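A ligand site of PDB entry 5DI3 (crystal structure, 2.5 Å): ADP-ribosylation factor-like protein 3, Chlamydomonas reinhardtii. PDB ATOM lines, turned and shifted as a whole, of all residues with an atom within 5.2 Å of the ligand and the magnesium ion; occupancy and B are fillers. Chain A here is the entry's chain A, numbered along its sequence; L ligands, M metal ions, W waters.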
ATOM      1  N   GLY A  23     -21.332 -12.253  28.746  1.00  0.00           N
ATOM      2  CA  GLY A  23     -22.040 -10.991  28.671  1.00  0.00           C
ATOM      3  C   GLY A  23     -23.509 -11.205  28.346  1.00  0.00           C
ATOM      4  O   GLY A  23     -23.894 -12.296  27.918  1.00  0.00           O
ATOM      5  N   LEU A  24     -24.325 -10.180  28.559  1.00  0.00           N
ATOM      6  CA  LEU A  24     -25.753 -10.250  28.271  1.00  0.00           C
ATOM      7  C   LEU A  24     -25.949 -10.552  26.801  1.00  0.00           C
ATOM      8  O   LEU A  24     -25.114 -10.190  25.974  1.00  0.00           O
ATOM      9  CB  LEU A  24     -26.458  -8.950  28.630  1.00  0.00           C
ATOM     10  CG  LEU A  24     -26.534  -8.491  30.082  1.00  0.00           C
ATOM     11  CD1 LEU A  24     -27.469  -7.286  30.182  1.00  0.00           C
ATOM     12  CD2 LEU A  24     -26.979  -9.605  31.010  1.00  0.00           C
ATOM     13  N   ASP A  25     -27.064 -11.210  26.475  1.00  0.00           N
ATOM     14  CA  ASP A  25     -27.456 -11.366  25.078  1.00  0.00           C
ATOM     15  C   ASP A  25     -27.535  -9.991  24.433  1.00  0.00           C
ATOM     16  O   ASP A  25     -27.896  -9.014  25.089  1.00  0.00           O
ATOM     17  CB  ASP A  25     -28.785 -12.107  24.959  1.00  0.00           C
ATOM     18  CG  ASP A  25     -29.959 -11.321  25.532  1.00  0.00           C
ATOM     19  OD1 ASP A  25     -30.096 -11.291  26.788  1.00  0.00           O
ATOM     20  OD2 ASP A  25     -30.722 -10.734  24.732  1.00  0.00           O
ATOM     21  N   ASN A  26     -27.166  -9.936  23.147  1.00  0.00           N
ATOM     22  CA  ASN A  26     -27.140  -8.713  22.339  1.00  0.00           C
ATOM     23  C   ASN A  26     -25.960  -7.783  22.613  1.00  0.00           C
ATOM     24  O   ASN A  26     -25.798  -6.769  21.934  1.00  0.00           O
ATOM     25  CB  ASN A  26     -28.451  -7.930  22.502  1.00  0.00           C
ATOM     26  CG  ASN A  26     -28.748  -7.037  21.312  1.00  0.00           C
ATOM     27  OD1 ASN A  26     -28.954  -7.520  20.192  1.00  0.00           O
ATOM     28  ND2 ASN A  26     -28.751  -5.721  21.541  1.00  0.00           N
ATOM     29  N   ALA A  27     -25.119  -8.124  23.591  1.00  0.00           N
ATOM     30  CA  ALA A  27     -23.977  -7.278  23.935  1.00  0.00           C
ATOM     31  C   ALA A  27     -22.963  -7.189  22.794  1.00  0.00           C
ATOM     32  O   ALA A  27     -22.278  -6.176  22.639  1.00  0.00           O
ATOM     33  CB  ALA A  27     -23.289  -7.776  25.184  1.00  0.00           C
ATOM     34  N   GLY A  28     -22.884  -8.248  21.987  1.00  0.00           N
ATOM     35  CA  GLY A  28     -21.996  -8.242  20.831  1.00  0.00           C
ATOM     36  C   GLY A  28     -20.849  -9.222  20.907  1.00  0.00           C
ATOM     37  O   GLY A  28     -19.846  -9.063  20.198  1.00  0.00           O
ATOM     38  N   LYS A  29     -20.984 -10.235  21.759  1.00  0.00           N
ATOM     39  CA  LYS A  29     -19.960 -11.256  21.939  1.00  0.00           C
ATOM     40  C   LYS A  29     -19.511 -11.878  20.609  1.00  0.00           C
ATOM     41  O   LYS A  29     -18.336 -11.797  20.248  1.00  0.00           O
ATOM     42  CB  LYS A  29     -20.461 -12.354  22.883  1.00  0.00           C
ATOM     43  CG  LYS A  29     -20.711 -11.874  24.307  1.00  0.00           C
ATOM     44  CD  LYS A  29     -21.145 -13.009  25.220  1.00  0.00           C
ATOM     45  CE  LYS A  29     -22.511 -13.575  24.823  1.00  0.00           C
ATOM     46  NZ  LYS A  29     -23.633 -12.622  25.058  1.00  0.00           N
ATOM     47  N   THR A  30     -20.452 -12.493  19.893  1.00  0.00           N
ATOM     48  CA  THR A  30     -20.159 -13.149  18.616  1.00  0.00           C
ATOM     49  C   THR A  30     -19.576 -12.190  17.568  1.00  0.00           C
ATOM     50  O   THR A  30     -18.621 -12.531  16.864  1.00  0.00           O
ATOM     51  CB  THR A  30     -21.423 -13.815  18.030  1.00  0.00           C
ATOM     52  OG1 THR A  30     -22.036 -14.647  19.029  1.00  0.00           O
ATOM     53  CG2 THR A  30     -21.085 -14.655  16.801  1.00  0.00           C
ATOM     54  N   THR A  31     -20.133 -10.991  17.485  1.00  0.00           N
ATOM     55  CA  THR A  31     -19.643  -9.993  16.529  1.00  0.00           C
ATOM     56  C   THR A  31     -18.176  -9.654  16.789  1.00  0.00           C
ATOM     57  O   THR A  31     -17.399  -9.499  15.854  1.00  0.00           O
ATOM     58  CB  THR A  31     -20.484  -8.717  16.581  1.00  0.00           C
ATOM     59  OG1 THR A  31     -21.872  -9.046  16.436  1.00  0.00           O
ATOM     60  CG2 THR A  31     -20.074  -7.764  15.463  1.00  0.00           C
ATOM     61  N   ILE A  41     -19.447 -10.187   9.429  1.00  0.00           N
ATOM     62  CA  ILE A  41     -20.347  -9.951  10.557  1.00  0.00           C
ATOM     63  C   ILE A  41     -21.675  -9.336  10.136  1.00  0.00           C
ATOM     64  O   ILE A  41     -22.466  -8.941  10.985  1.00  0.00           O
ATOM     65  CB  ILE A  41     -19.694  -9.007  11.597  1.00  0.00           C
ATOM     66  CG1 ILE A  41     -19.279  -7.690  10.925  1.00  0.00           C
ATOM     67  CG2 ILE A  41     -18.509  -9.679  12.256  1.00  0.00           C
ATOM     68  CD1 ILE A  41     -18.469  -6.776  11.826  1.00  0.00           C
ATOM     69  N   ILE A  44     -25.598 -11.804  11.584  1.00  0.00           N
ATOM     70  CA  ILE A  44     -25.276 -12.574  12.775  1.00  0.00           C
ATOM     71  C   ILE A  44     -26.561 -12.933  13.496  1.00  0.00           C
ATOM     72  O   ILE A  44     -27.548 -12.190  13.472  1.00  0.00           O
ATOM     73  CB  ILE A  44     -24.280 -11.809  13.684  1.00  0.00           C
ATOM     74  CG1 ILE A  44     -22.872 -11.889  13.095  1.00  0.00           C
ATOM     75  CG2 ILE A  44     -24.277 -12.350  15.117  1.00  0.00           C
ATOM     76  CD1 ILE A  44     -21.759 -11.596  14.068  1.00  0.00           C
ATOM     77  N   THR A  45     -26.548 -14.106  14.119  1.00  0.00           N
ATOM     78  CA  THR A  45     -27.697 -14.718  14.742  1.00  0.00           C
ATOM     79  C   THR A  45     -27.443 -14.808  16.249  1.00  0.00           C
ATOM     80  O   THR A  45     -26.294 -14.985  16.649  1.00  0.00           O
ATOM     81  CB  THR A  45     -27.928 -16.116  14.147  1.00  0.00           C
ATOM     82  OG1 THR A  45     -28.240 -15.964  12.753  1.00  0.00           O
ATOM     83  CG2 THR A  45     -29.054 -16.863  14.838  1.00  0.00           C
ATOM     84  N   PRO A  46     -28.491 -14.681  17.078  1.00  0.00           N
ATOM     85  CA  PRO A  46     -28.294 -14.995  18.501  1.00  0.00           C
ATOM     86  C   PRO A  46     -27.772 -16.419  18.661  1.00  0.00           C
ATOM     87  O   PRO A  46     -28.059 -17.284  17.844  1.00  0.00           O
ATOM     88  CB  PRO A  46     -29.702 -14.845  19.098  1.00  0.00           C
ATOM     89  CG  PRO A  46     -30.373 -13.849  18.198  1.00  0.00           C
ATOM     90  CD  PRO A  46     -29.832 -14.114  16.817  1.00  0.00           C
ATOM     91  N   THR A  47     -26.995 -16.649  19.714  1.00  0.00           N
ATOM     92  CA  THR A  47     -26.218 -17.882  19.812  1.00  0.00           C
ATOM     93  C   THR A  47     -26.854 -18.910  20.741  1.00  0.00           C
ATOM     94  O   THR A  47     -27.328 -18.586  21.833  1.00  0.00           O
ATOM     95  CB  THR A  47     -24.772 -17.552  20.280  1.00  0.00           C
ATOM     96  OG1 THR A  47     -24.063 -16.938  19.197  1.00  0.00           O
ATOM     97  CG2 THR A  47     -24.012 -18.790  20.707  1.00  0.00           C
ATOM     98  N   ASP A  66     -17.838 -19.734  22.101  1.00  0.00           N
ATOM     99  CA  ASP A  66     -18.830 -18.702  21.831  1.00  0.00           C
ATOM    100  C   ASP A  66     -20.175 -19.204  22.329  1.00  0.00           C
ATOM    101  O   ASP A  66     -20.670 -20.246  21.883  1.00  0.00           O
ATOM    102  CB  ASP A  66     -18.880 -18.346  20.348  1.00  0.00           C
ATOM    103  CG  ASP A  66     -19.729 -17.114  20.068  1.00  0.00           C
ATOM    104  OD1 ASP A  66     -19.878 -16.280  20.980  1.00  0.00           O
ATOM    105  OD2 ASP A  66     -20.234 -16.987  18.937  1.00  0.00           O
ATOM    106  N   ILE A  67     -20.756 -18.473  23.268  1.00  0.00           N
ATOM    107  CA  ILE A  67     -21.935 -18.925  24.003  1.00  0.00           C
ATOM    108  C   ILE A  67     -23.013 -17.833  23.979  1.00  0.00           C
ATOM    109  O   ILE A  67     -22.698 -16.650  23.905  1.00  0.00           O
ATOM    110  CB  ILE A  67     -21.581 -19.265  25.478  1.00  0.00           C
ATOM    111  CG1 ILE A  67     -20.318 -20.124  25.532  1.00  0.00           C
ATOM    112  CG2 ILE A  67     -22.735 -19.966  26.176  1.00  0.00           C
ATOM    113  CD1 ILE A  67     -19.875 -20.465  26.938  1.00  0.00           C
ATOM    114  N   GLY A  68     -24.279 -18.238  24.046  1.00  0.00           N
ATOM    115  CA  GLY A  68     -25.373 -17.288  24.112  1.00  0.00           C
ATOM    116  C   GLY A  68     -25.533 -16.670  25.481  1.00  0.00           C
ATOM    117  O   GLY A  68     -25.203 -17.283  26.497  1.00  0.00           O
ATOM    118  N   GLY A  69     -26.036 -15.440  25.518  1.00  0.00           N
ATOM    119  CA  GLY A  69     -26.224 -14.725  26.761  1.00  0.00           C
ATOM    120  C   GLY A  69     -27.670 -14.460  27.139  1.00  0.00           C
ATOM    121  O   GLY A  69     -27.964 -13.529  27.889  1.00  0.00           O
ATOM    122  N   GLN A  70     -28.577 -15.277  26.601  1.00  0.00           N
ATOM    123  CA  GLN A  70     -29.976 -15.174  26.968  1.00  0.00           C
ATOM    124  C   GLN A  70     -30.147 -15.732  28.373  1.00  0.00           C
ATOM    125  O   GLN A  70     -29.356 -16.555  28.826  1.00  0.00           O
ATOM    126  CB  GLN A  70     -30.863 -15.927  25.973  1.00  0.00           C
ATOM    127  CG  GLN A  70     -31.544 -15.018  24.974  1.00  0.00           C
ATOM    128  CD  GLN A  70     -32.173 -15.774  23.822  1.00  0.00           C
ATOM    129  OE1 GLN A  70     -32.984 -16.671  24.026  1.00  0.00           O
ATOM    130  NE2 GLN A  70     -31.784 -15.419  22.601  1.00  0.00           N
ATOM    131  N   ASN A 125     -18.593  -2.219  24.381  1.00  0.00           N
ATOM    132  CA  ASN A 125     -18.890  -2.315  22.953  1.00  0.00           C
ATOM    133  C   ASN A 125     -19.941  -1.324  22.475  1.00  0.00           C
ATOM    134  O   ASN A 125     -20.700  -0.788  23.290  1.00  0.00           O
ATOM    135  CB  ASN A 125     -19.335  -3.745  22.630  1.00  0.00           C
ATOM    136  CG  ASN A 125     -19.232  -4.072  21.138  1.00  0.00           C
ATOM    137  OD1 ASN A 125     -18.345  -3.579  20.433  1.00  0.00           O
ATOM    138  ND2 ASN A 125     -20.142  -4.922  20.663  1.00  0.00           N
ATOM    139  N   LYS A 126     -19.980  -1.099  21.170  1.00  0.00           N
ATOM    140  CA  LYS A 126     -20.950  -0.229  20.493  1.00  0.00           C
ATOM    141  C   LYS A 126     -20.721   1.239  20.814  1.00  0.00           C
ATOM    142  O   LYS A 126     -21.677   1.999  20.997  1.00  0.00           O
ATOM    143  CB  LYS A 126     -22.387  -0.637  20.834  1.00  0.00           C
ATOM    144  CG  LYS A 126     -22.734  -2.043  20.410  1.00  0.00           C
ATOM    145  CD  LYS A 126     -24.156  -2.430  20.786  1.00  0.00           C
ATOM    146  CE  LYS A 126     -24.430  -3.898  20.458  1.00  0.00           C
ATOM    147  NZ  LYS A 126     -25.801  -4.324  20.864  1.00  0.00           N
ATOM    148  N   ASP A 128     -19.910   3.234  18.800  1.00  0.00           N
ATOM    149  CA  ASP A 128     -20.328   3.926  17.582  1.00  0.00           C
ATOM    150  C   ASP A 128     -21.771   4.414  17.695  1.00  0.00           C
ATOM    151  O   ASP A 128     -22.237   5.179  16.845  1.00  0.00           O
ATOM    152  CB  ASP A 128     -20.180   2.993  16.386  1.00  0.00           C
ATOM    153  CG  ASP A 128     -20.966   1.702  16.547  1.00  0.00           C
ATOM    154  OD1 ASP A 128     -20.526   0.834  17.337  1.00  0.00           O
ATOM    155  OD2 ASP A 128     -22.026   1.570  15.902  1.00  0.00           O
ATOM    156  N   LEU A 129     -22.482   3.957  18.722  1.00  0.00           N
ATOM    157  CA  LEU A 129     -23.868   4.364  18.932  1.00  0.00           C
ATOM    158  C   LEU A 129     -23.969   5.645  19.737  1.00  0.00           C
ATOM    159  O   LEU A 129     -23.223   5.839  20.698  1.00  0.00           O
ATOM    160  CB  LEU A 129     -24.649   3.251  19.624  1.00  0.00           C
ATOM    161  CG  LEU A 129     -24.786   1.938  18.848  1.00  0.00           C
ATOM    162  CD1 LEU A 129     -25.690   0.959  19.575  1.00  0.00           C
ATOM    163  CD2 LEU A 129     -25.294   2.214  17.433  1.00  0.00           C
ATOM    164  N   CYS A 157     -14.765  -0.065  22.692  1.00  0.00           N
ATOM    165  CA  CYS A 157     -14.593  -0.661  21.382  1.00  0.00           C
ATOM    166  C   CYS A 157     -15.865  -0.606  20.554  1.00  0.00           C
ATOM    167  O   CYS A 157     -16.943  -0.330  21.078  1.00  0.00           O
ATOM    168  CB  CYS A 157     -14.140  -2.115  21.519  1.00  0.00           C
ATOM    169  SG  CYS A 157     -15.415  -3.204  22.192  1.00  0.00           S
ATOM    170  N   SER A 158     -15.719  -0.868  19.263  1.00  0.00           N
ATOM    171  CA  SER A 158     -16.852  -1.012  18.371  1.00  0.00           C
ATOM    172  C   SER A 158     -16.569  -2.186  17.449  1.00  0.00           C
ATOM    173  O   SER A 158     -15.726  -2.090  16.542  1.00  0.00           O
ATOM    174  CB  SER A 158     -17.090   0.267  17.565  1.00  0.00           C
ATOM    175  OG  SER A 158     -18.125   0.081  16.602  1.00  0.00           O
ATOM    176  N   ALA A 159     -17.240  -3.299  17.683  1.00  0.00           N
ATOM    177  CA  ALA A 159     -17.060  -4.488  16.869  1.00  0.00           C
ATOM    178  C   ALA A 159     -17.540  -4.219  15.446  1.00  0.00           C
ATOM    179  O   ALA A 159     -16.958  -4.702  14.482  1.00  0.00           O
ATOM    180  CB  ALA A 159     -17.793  -5.682  17.471  1.00  0.00           C
ATOM    181  N   LYS A 160     -18.607  -3.422  15.346  1.00  0.00           N
ATOM    182  CA  LYS A 160     -19.175  -3.028  14.055  1.00  0.00           C
ATOM    183  C   LYS A 160     -18.142  -2.336  13.164  1.00  0.00           C
ATOM    184  O   LYS A 160     -18.150  -2.497  11.949  1.00  0.00           O
ATOM    185  CB  LYS A 160     -20.372  -2.094  14.275  1.00  0.00           C
ATOM    186  CG  LYS A 160     -21.153  -1.759  13.017  1.00  0.00           C
ATOM    187  CD  LYS A 160     -22.295  -0.812  13.345  1.00  0.00           C
ATOM    188  CE  LYS A 160     -23.404  -0.885  12.306  1.00  0.00           C
ATOM    189  NZ  LYS A 160     -22.965  -0.369  10.978  1.00  0.00           N
ATOM    190  N   GLN A 161     -17.239  -1.576  13.785  1.00  0.00           N
ATOM    191  CA  GLN A 161     -16.300  -0.747  13.033  1.00  0.00           C
ATOM    192  C   GLN A 161     -14.845  -1.196  13.190  1.00  0.00           C
ATOM    193  O   GLN A 161     -13.944  -0.567  12.625  1.00  0.00           O
ATOM    194  CB  GLN A 161     -16.437   0.711  13.443  1.00  0.00           C
ATOM    195  CG  GLN A 161     -17.576   1.441  12.733  1.00  0.00           C
ATOM    196  CD  GLN A 161     -18.114   2.608  13.522  1.00  0.00           C
ATOM    197  OE1 GLN A 161     -17.458   3.124  14.442  1.00  0.00           O
ATOM    198  NE2 GLN A 161     -19.330   3.050  13.185  1.00  0.00           N
HETATM  199  P1  LIG L   1     -26.117 -13.575  22.067  1.00  0.00           P
HETATM  200  O1  LIG L   1     -25.406 -14.527  21.132  1.00  0.00           O
HETATM  201  O2  LIG L   1     -25.670 -13.642  23.510  1.00  0.00           O
HETATM  202  O3  LIG L   1     -27.588 -13.822  21.887  1.00  0.00           O
HETATM  203  N1  LIG L   1     -25.784 -12.117  21.537  1.00  0.00           N
HETATM  204  P2  LIG L   1     -24.306 -11.573  21.274  1.00  0.00           P
HETATM  205  O4  LIG L   1     -23.558 -12.574  20.483  1.00  0.00           O
HETATM  206  O5  LIG L   1     -23.716 -11.170  22.579  1.00  0.00           O
HETATM  207  O6  LIG L   1     -24.394 -10.319  20.414  1.00  0.00           O
HETATM  208  P3  LIG L   1     -24.409 -10.342  18.873  1.00  0.00           P
HETATM  209  O7  LIG L   1     -25.412 -11.349  18.464  1.00  0.00           O
HETATM  210  O8  LIG L   1     -23.048 -10.440  18.289  1.00  0.00           O
HETATM  211  O9  LIG L   1     -24.933  -8.936  18.420  1.00  0.00           O
HETATM  212  C1  LIG L   1     -26.223  -8.435  18.760  1.00  0.00           C
HETATM  213  C2  LIG L   1     -26.549  -7.221  17.900  1.00  0.00           C
HETATM  214  O10 LIG L   1     -25.593  -6.163  18.168  1.00  0.00           O
HETATM  215  C3  LIG L   1     -26.448  -7.462  16.390  1.00  0.00           C
HETATM  216  O11 LIG L   1     -27.345  -6.592  15.741  1.00  0.00           O
HETATM  217  C4  LIG L   1     -25.009  -7.047  16.123  1.00  0.00           C
HETATM  218  O12 LIG L   1     -24.720  -6.788  14.759  1.00  0.00           O
HETATM  219  C5  LIG L   1     -24.991  -5.779  16.943  1.00  0.00           C
HETATM  220  N2  LIG L   1     -23.654  -5.261  17.208  1.00  0.00           N
HETATM  221  C6  LIG L   1     -22.535  -5.978  17.564  1.00  0.00           C
HETATM  222  N3  LIG L   1     -21.476  -5.238  17.722  1.00  0.00           N
HETATM  223  C7  LIG L   1     -21.904  -3.941  17.452  1.00  0.00           C
HETATM  224  C8  LIG L   1     -21.195  -2.716  17.470  1.00  0.00           C
HETATM  225  O13 LIG L   1     -19.996  -2.511  17.723  1.00  0.00           O
HETATM  226  N4  LIG L   1     -22.023  -1.642  17.126  1.00  0.00           N
HETATM  227  C9  LIG L   1     -23.360  -1.753  16.816  1.00  0.00           C
HETATM  228  N5  LIG L   1     -23.983  -0.611  16.517  1.00  0.00           N
HETATM  229  N6  LIG L   1     -24.043  -2.897  16.809  1.00  0.00           N
HETATM  230  C10 LIG L   1     -23.246  -3.947  17.135  1.00  0.00           C
HETATM  231 MG    MG M   1     -23.609 -14.935  20.422  1.00  0.00          MG
HETATM  232  O   HOH W   1     -21.829 -15.418  21.819  1.00  0.00           O
HETATM  233  O   HOH W   2     -24.512 -13.908  18.540  1.00  0.00           O
HETATM  234  O   HOH W   3     -28.349 -16.280  22.673  1.00  0.00           O
HETATM  235  O   HOH W   4     -29.226 -11.969  21.183  1.00  0.00           O
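The backbone carbonyl oxygen of Gly 69 is in hydrogen-bond range of the backbone NH of Asp 25 (2.9 Å). The backbone carbonyl oxygen (O) of Leu 24 sits at hydrogen-bond distance from the side-chain amino group (NZ) of Lys 29 (3.0 Å). O of Gly 23 is in hydrogen-bond range of NZ of Lys 29, at 2.9 Å. The backbone NH of Ala 159 is in hydrogen-bond range of the side-chain amide oxygen of Asn 125 (3.0 Å). The side-chain hydroxyl (OG) of Ser 158 lies within hydrogen-bond range of the side-chain carboxylate (OD1) of Asp 128 (2.6 Å). The backbone carbonyl oxygen of Ala 27 sits at hydrogen-bond distance from the side-chain amide nitrogen of Asn 125, 3.2 Å away. The backbone carbonyl oxygen of Cys 157 sits at hydrogen-bond distance from the backbone NH of Lys 126, 3.1 Å away. OG of Ser 158 is in hydrogen-bond range of N of Gln 161 (3.4 Å).
Merely in contact with the magnesium ion: Ile 67 (3.99 Å). Three residues have an atom within 4 Å of the magnesium ion: Thr 30, Thr 47 and Ile 67. The nearest printed residue that does not touch the magnesium ion is Asp 66 (4.01 Å).
Water W2 bridges O7 of the ligand (2.7 Å) and O of Thr 45 (2.8 Å). Water W4 bridges O3 of the ligand and N of Asn 26. Water W3 lies within hydrogen-bond range of the backbone carbonyl oxygen of Thr 47 (2.7 Å) and an oxygen (O3) of the ligand (2.7 Å).
The backbone NH (N) of Thr 30 lies close to an oxygen (O4) of the ligand (3.2 Å). N of Thr 47 lies close to O1 of the ligand (3.0 Å). N of Thr 31 lies within hydrogen-bond range of O8 of the ligand, at 3.1 Å. An oxygen (O8) of the ligand lies within hydrogen-bond range of the side-chain hydroxyl (OG1) of Thr 31, at 2.6 Å. N of Gly 69 sits at hydrogen-bond distance from O2 of the ligand (2.7 Å). The backbone NH of Lys 29 sits at hydrogen-bond distance from an oxygen (O5) of the ligand (3.0 Å). The side-chain amino group (NZ) of Lys 29 lies within salt-bridge range of an oxygen (O2) of the ligand, at 2.8 Å. O13 of the ligand is in hydrogen-bond range of N of Ala 159 (2.9 Å). The backbone NH of Lys 160 lies within hydrogen-bond range of an oxygen (O13) of the ligand (2.9 Å). The side-chain carboxylate (OD1) of Asp 128 sits at hydrogen-bond distance from a nitrogen (N4) of the ligand (2.9 Å). N of Gly 28 lies within hydrogen-bond range of O6 of the ligand (3.0 Å). N3 of the ligand sits at hydrogen-bond distance from ND2 of Asn 125 (3.2 Å). An oxygen (O10) of the ligand sits at hydrogen-bond distance from the side-chain amino group of Lys 126, 3.3 Å away. The side-chain hydroxyl (OG) of Ser 158 is in hydrogen-bond range of an oxygen (O13) of the ligand (3.4 Å).
The magnesium ion is bound by an oxygen (O1) of the ligand (2.0 Å), the side-chain hydroxyl (OG1) of Thr 30 (2.1 Å), water W1 (2.3 Å), water W2 (2.3 Å), an oxygen (O4) of the ligand (2.4 Å) and the side-chain hydroxyl (OG1) of Thr 47 (2.4 Å). The magnesium ion has six donor atoms within binding distance.
N of Asn 26 sits close to N1 of the ligand, 3.0 Å away. Leu 24 touches the ligand. CA of Asp 25 touches O2 of the ligand, at 3.3 Å. Ala 27 touches the ligand (N to O5, 3.5 Å). CG2 of Ile 44 touches O7 of the ligand, at 3.7 Å. CB of Pro 46 touches O3 of the ligand, 3.6 Å away. Gly 68 touches the ligand. Leu 129 touches the ligand (CD2 to N5, 3.2 Å). Hydrophobic or aromatic side chains within 4 Å of the ligand: Ile 44, Pro 46, Leu 129 and Ala 159. The nearest printed residue that does not touch the ligand is Thr 45 (4.2 Å).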
